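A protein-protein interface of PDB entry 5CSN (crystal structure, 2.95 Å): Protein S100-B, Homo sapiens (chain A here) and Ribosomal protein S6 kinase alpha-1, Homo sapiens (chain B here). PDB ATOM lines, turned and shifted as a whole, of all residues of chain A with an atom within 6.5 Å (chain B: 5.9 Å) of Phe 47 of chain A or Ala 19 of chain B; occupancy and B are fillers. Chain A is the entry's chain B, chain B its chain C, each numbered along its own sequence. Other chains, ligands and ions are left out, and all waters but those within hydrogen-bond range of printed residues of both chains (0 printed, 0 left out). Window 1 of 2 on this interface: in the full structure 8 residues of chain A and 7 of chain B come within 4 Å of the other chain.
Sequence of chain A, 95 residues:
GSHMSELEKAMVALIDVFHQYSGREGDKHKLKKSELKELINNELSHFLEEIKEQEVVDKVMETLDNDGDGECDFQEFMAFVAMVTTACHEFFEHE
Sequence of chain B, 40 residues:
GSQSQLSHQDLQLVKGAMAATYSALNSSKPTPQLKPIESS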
ATOM      1  N   GLU A  43      -8.319  15.026  17.626  1.00  0.00           N
ATOM      2  CA  GLU A  43      -9.483  14.329  17.083  1.00  0.00           C
ATOM      3  C   GLU A  43      -9.937  14.828  15.710  1.00  0.00           C
ATOM      4  O   GLU A  43     -10.710  14.155  15.037  1.00  0.00           O
ATOM      5  CB  GLU A  43     -10.652  14.424  18.070  1.00  0.00           C
ATOM      6  CG  GLU A  43     -10.277  14.141  19.521  1.00  0.00           C
ATOM      7  CD  GLU A  43      -9.810  12.711  19.756  1.00  0.00           C
ATOM      8  OE1 GLU A  43     -10.076  11.838  18.903  1.00  0.00           O
ATOM      9  OE2 GLU A  43      -9.174  12.460  20.800  1.00  0.00           O
ATOM     10  N   LEU A  44      -9.463  16.000  15.297  1.00  0.00           N
ATOM     11  CA  LEU A  44      -9.798  16.533  13.974  1.00  0.00           C
ATOM     12  C   LEU A  44      -8.570  16.752  13.087  1.00  0.00           C
ATOM     13  O   LEU A  44      -8.551  17.661  12.258  1.00  0.00           O
ATOM     14  CB  LEU A  44     -10.585  17.838  14.113  1.00  0.00           C
ATOM     15  CG  LEU A  44     -11.976  17.705  14.740  1.00  0.00           C
ATOM     16  CD1 LEU A  44     -12.601  19.071  14.966  1.00  0.00           C
ATOM     17  CD2 LEU A  44     -12.876  16.844  13.865  1.00  0.00           C
ATOM     18  N   SER A  45      -7.553  15.918  13.266  1.00  0.00           N
ATOM     19  CA  SER A  45      -6.277  16.078  12.570  1.00  0.00           C
ATOM     20  C   SER A  45      -6.320  15.731  11.078  1.00  0.00           C
ATOM     21  O   SER A  45      -5.294  15.787  10.399  1.00  0.00           O
ATOM     22  CB  SER A  45      -5.202  15.230  13.252  1.00  0.00           C
ATOM     23  OG  SER A  45      -5.437  13.847  13.045  1.00  0.00           O
ATOM     24  N   HIS A  46      -7.495  15.376  10.571  1.00  0.00           N
ATOM     25  CA  HIS A  46      -7.653  15.104   9.142  1.00  0.00           C
ATOM     26  C   HIS A  46      -8.572  16.103   8.449  1.00  0.00           C
ATOM     27  O   HIS A  46      -8.572  16.215   7.223  1.00  0.00           O
ATOM     28  CB  HIS A  46      -8.195  13.690   8.936  1.00  0.00           C
ATOM     29  CG  HIS A  46      -7.268  12.615   9.408  1.00  0.00           C
ATOM     30  ND1 HIS A  46      -7.390  12.020  10.645  1.00  0.00           N
ATOM     31  CD2 HIS A  46      -6.193  12.040   8.819  1.00  0.00           C
ATOM     32  CE1 HIS A  46      -6.438  11.117  10.793  1.00  0.00           C
ATOM     33  NE2 HIS A  46      -5.698  11.110   9.699  1.00  0.00           N
ATOM     34  N   PHE A  47      -9.352  16.826   9.241  1.00  0.00           N
ATOM     35  CA  PHE A  47     -10.317  17.782   8.714  1.00  0.00           C
ATOM     36  C   PHE A  47      -9.841  19.223   8.885  1.00  0.00           C
ATOM     37  O   PHE A  47     -10.071  20.064   8.018  1.00  0.00           O
ATOM     38  CB  PHE A  47     -11.682  17.582   9.379  1.00  0.00           C
ATOM     39  CG  PHE A  47     -12.357  16.289   9.004  1.00  0.00           C
ATOM     40  CD1 PHE A  47     -11.852  15.494   7.986  1.00  0.00           C
ATOM     41  CD2 PHE A  47     -13.496  15.868   9.669  1.00  0.00           C
ATOM     42  CE1 PHE A  47     -12.469  14.307   7.638  1.00  0.00           C
ATOM     43  CE2 PHE A  47     -14.118  14.680   9.327  1.00  0.00           C
ATOM     44  CZ  PHE A  47     -13.604  13.899   8.311  1.00  0.00           C
ATOM     45  N   LEU A  48      -9.172  19.502   9.999  1.00  0.00           N
ATOM     46  CA  LEU A  48      -8.714  20.856  10.298  1.00  0.00           C
ATOM     47  C   LEU A  48      -7.194  20.920  10.419  1.00  0.00           C
ATOM     48  O   LEU A  48      -6.566  19.989  10.923  1.00  0.00           O
ATOM     49  CB  LEU A  48      -9.347  21.357  11.597  1.00  0.00           C
ATOM     50  CG  LEU A  48     -10.872  21.442  11.661  1.00  0.00           C
ATOM     51  CD1 LEU A  48     -11.300  21.935  13.031  1.00  0.00           C
ATOM     52  CD2 LEU A  48     -11.415  22.346  10.567  1.00  0.00           C
ATOM     53  N   GLU A  49      -6.609  22.022   9.956  1.00  0.00           N
ATOM     54  CA  GLU A  49      -5.166  22.218  10.059  1.00  0.00           C
ATOM     55  C   GLU A  49      -4.754  22.317  11.519  1.00  0.00           C
ATOM     56  O   GLU A  49      -5.440  22.954  12.318  1.00  0.00           O
ATOM     57  CB  GLU A  49      -4.725  23.484   9.322  1.00  0.00           C
ATOM     58  CG  GLU A  49      -4.824  23.424   7.811  1.00  0.00           C
ATOM     59  CD  GLU A  49      -4.451  24.744   7.164  1.00  0.00           C
ATOM     60  OE1 GLU A  49      -3.369  25.278   7.484  1.00  0.00           O
ATOM     61  OE2 GLU A  49      -5.246  25.252   6.344  1.00  0.00           O
ATOM     62  N   VAL A  84     -18.033  22.262  10.578  1.00  0.00           N
ATOM     63  CA  VAL A  84     -17.017  21.360  10.044  1.00  0.00           C
ATOM     64  C   VAL A  84     -17.611  20.276   9.142  1.00  0.00           C
ATOM     65  O   VAL A  84     -17.097  20.014   8.055  1.00  0.00           O
ATOM     66  CB  VAL A  84     -16.221  20.691  11.187  1.00  0.00           C
ATOM     67  CG1 VAL A  84     -15.327  19.586  10.648  1.00  0.00           C
ATOM     68  CG2 VAL A  84     -15.393  21.727  11.930  1.00  0.00           C
ATOM     69  N   THR A  85     -18.704  19.666   9.591  1.00  0.00           N
ATOM     70  CA  THR A  85     -19.351  18.584   8.851  1.00  0.00           C
ATOM     71  C   THR A  85     -19.861  19.064   7.494  1.00  0.00           C
ATOM     72  O   THR A  85     -19.688  18.383   6.484  1.00  0.00           O
ATOM     73  CB  THR A  85     -20.522  17.977   9.647  1.00  0.00           C
ATOM     74  OG1 THR A  85     -20.077  17.620  10.962  1.00  0.00           O
ATOM     75  CG2 THR A  85     -21.055  16.742   8.947  1.00  0.00           C
ATOM     76  N   ALA A  87     -18.765  21.508   5.666  1.00  0.00           N
ATOM     77  CA  ALA A  87     -17.580  21.732   4.833  1.00  0.00           C
ATOM     78  C   ALA A  87     -17.052  20.444   4.194  1.00  0.00           C
ATOM     79  O   ALA A  87     -16.670  20.423   3.025  1.00  0.00           O
ATOM     80  CB  ALA A  87     -16.487  22.395   5.654  1.00  0.00           C
ATOM     81  N   CYS A  88     -17.046  19.375   4.981  1.00  0.00           N
ATOM     82  CA  CYS A  88     -16.613  18.044   4.552  1.00  0.00           C
ATOM     83  C   CYS A  88     -17.535  17.443   3.491  1.00  0.00           C
ATOM     84  O   CYS A  88     -17.091  16.677   2.637  1.00  0.00           O
ATOM     85  CB  CYS A  88     -16.515  17.106   5.755  1.00  0.00           C
ATOM     86  SG  CYS A  88     -15.344  17.657   7.017  1.00  0.00           S
ATOM     87  N   ALA B  17      -8.340  16.575   2.545  1.00  0.00           N
ATOM     88  CA  ALA B  17      -7.358  17.510   3.079  1.00  0.00           C
ATOM     89  C   ALA B  17      -7.194  18.727   2.170  1.00  0.00           C
ATOM     90  O   ALA B  17      -6.974  18.577   0.969  1.00  0.00           O
ATOM     91  CB  ALA B  17      -6.017  16.816   3.274  1.00  0.00           C
ATOM     92  N   MET B  18      -7.308  19.931   2.729  1.00  0.00           N
ATOM     93  CA  MET B  18      -7.626  20.144   4.140  1.00  0.00           C
ATOM     94  C   MET B  18      -8.397  21.452   4.285  1.00  0.00           C
ATOM     95  O   MET B  18      -8.445  22.255   3.353  1.00  0.00           O
ATOM     96  CB  MET B  18      -6.353  20.177   4.994  1.00  0.00           C
ATOM     97  CG  MET B  18      -6.561  19.769   6.445  1.00  0.00           C
ATOM     98  SD  MET B  18      -5.006  19.448   7.300  1.00  0.00           S
ATOM     99  CE  MET B  18      -4.378  18.060   6.355  1.00  0.00           C
ATOM    100  N   ALA B  19      -9.002  21.669   5.449  1.00  0.00           N
ATOM    101  CA  ALA B  19      -9.737  22.903   5.699  1.00  0.00           C
ATOM    102  C   ALA B  19      -8.918  23.864   6.550  1.00  0.00           C
ATOM    103  O   ALA B  19      -7.770  23.584   6.884  1.00  0.00           O
ATOM    104  CB  ALA B  19     -11.067  22.606   6.368  1.00  0.00           C
ATOM    105  N   ALA B  20      -9.522  24.997   6.894  1.00  0.00           N
ATOM    106  CA  ALA B  20      -8.882  26.010   7.725  1.00  0.00           C
ATOM    107  C   ALA B  20      -9.949  26.914   8.321  1.00  0.00           C
ATOM    108  O   ALA B  20     -11.143  26.686   8.114  1.00  0.00           O
ATOM    109  CB  ALA B  20      -7.878  26.818   6.913  1.00  0.00           C
ATOM    110  N   THR B  21      -9.532  27.941   9.057  1.00  0.00           N
ATOM    111  CA  THR B  21     -10.477  28.940   9.557  1.00  0.00           C
ATOM    112  C   THR B  21     -10.964  29.754   8.362  1.00  0.00           C
ATOM    113  O   THR B  21     -11.990  30.428   8.425  1.00  0.00           O
ATOM    114  CB  THR B  21      -9.850  29.869  10.621  1.00  0.00           C
ATOM    115  OG1 THR B  21     -10.862  30.309  11.532  1.00  0.00           O
ATOM    116  CG2 THR B  21      -9.167  31.074   9.976  1.00  0.00           C
ATOM    117  N   SER B  23     -12.109  28.305   5.472  1.00  0.00           N
ATOM    118  CA  SER B  23     -13.336  27.608   5.115  1.00  0.00           C
ATOM    119  C   SER B  23     -14.315  27.500   6.277  1.00  0.00           C
ATOM    120  O   SER B  23     -15.528  27.372   6.082  1.00  0.00           O
ATOM    121  CB  SER B  23     -13.019  26.201   4.595  1.00  0.00           C
ATOM    122  OG  SER B  23     -12.093  26.245   3.522  1.00  0.00           O
ATOM    123  N   ALA B  24     -13.772  27.511   7.490  1.00  0.00           N
ATOM    124  CA  ALA B  24     -14.591  27.424   8.692  1.00  0.00           C
ATOM    125  C   ALA B  24     -15.411  28.696   8.834  1.00  0.00           C
ATOM    126  O   ALA B  24     -16.626  28.630   9.034  1.00  0.00           O
ATOM    127  CB  ALA B  24     -13.734  27.175   9.919  1.00  0.00           C
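The side-chain carboxylate of Glu 49 of chain A lies close to the backbone carbonyl oxygen of Ala 19 of chain B, 3.1 Å away.
The backbone NH (N) of Ala 19 of chain B sits close to the backbone carbonyl oxygen (O) of Phe 47 of chain A (3.2 Å).
Hydrophobic or aromatic side chains of chain B that line the printed part of chain A: Met 18, Ala 19 and Ala 20.
Along chain B the printed residues that touch a printed residue of chain A span positions 18 to 20.
Of the 11 printed residues of chain A, 3 touch a printed residue of chain B.
Printed residues of chain A that touch a printed residue of chain B: Phe 47, Leu 48 and Glu 49.
Phe 47 of chain A touches just these residues of chain B: Met 18 (3.9 Å) and Ala 19 (3.2 Å).
Of the printed residues of chain B, Leu 48 of chain A touches Met 18 (3.98 Å).
Printed residues of chain B within 4 Å of Glu 49 of chain A: Met 18, Ala 19 and Ala 20.
Of the printed residues of chain A, Met 18 of chain B touches Phe 47, Leu 48 and Glu 49.
Of the printed residues of chain A, Ala 19 of chain B touches Phe 47 (3.2 Å) and Glu 49 (3.1 Å).
Printed residues of chain A within 4 Å of Ala 20 of chain B: Glu 49 (3.1 Å).
The nearest residue of chain B that does not touch Phe 47 of chain A is Ala 20 of chain B (5.1 Å).
Among the printed residues, pairs that only touch across the chains: Glu 49 of chain A with Ala 20 of chain B (3.1 Å), Phe 47 of chain A with Met 18 of chain B (3.9 Å), Glu 49 of chain A with Met 18 of chain B (3.9 Å) and Leu 48 of chain A with Met 18 of chain B (3.98 Å).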
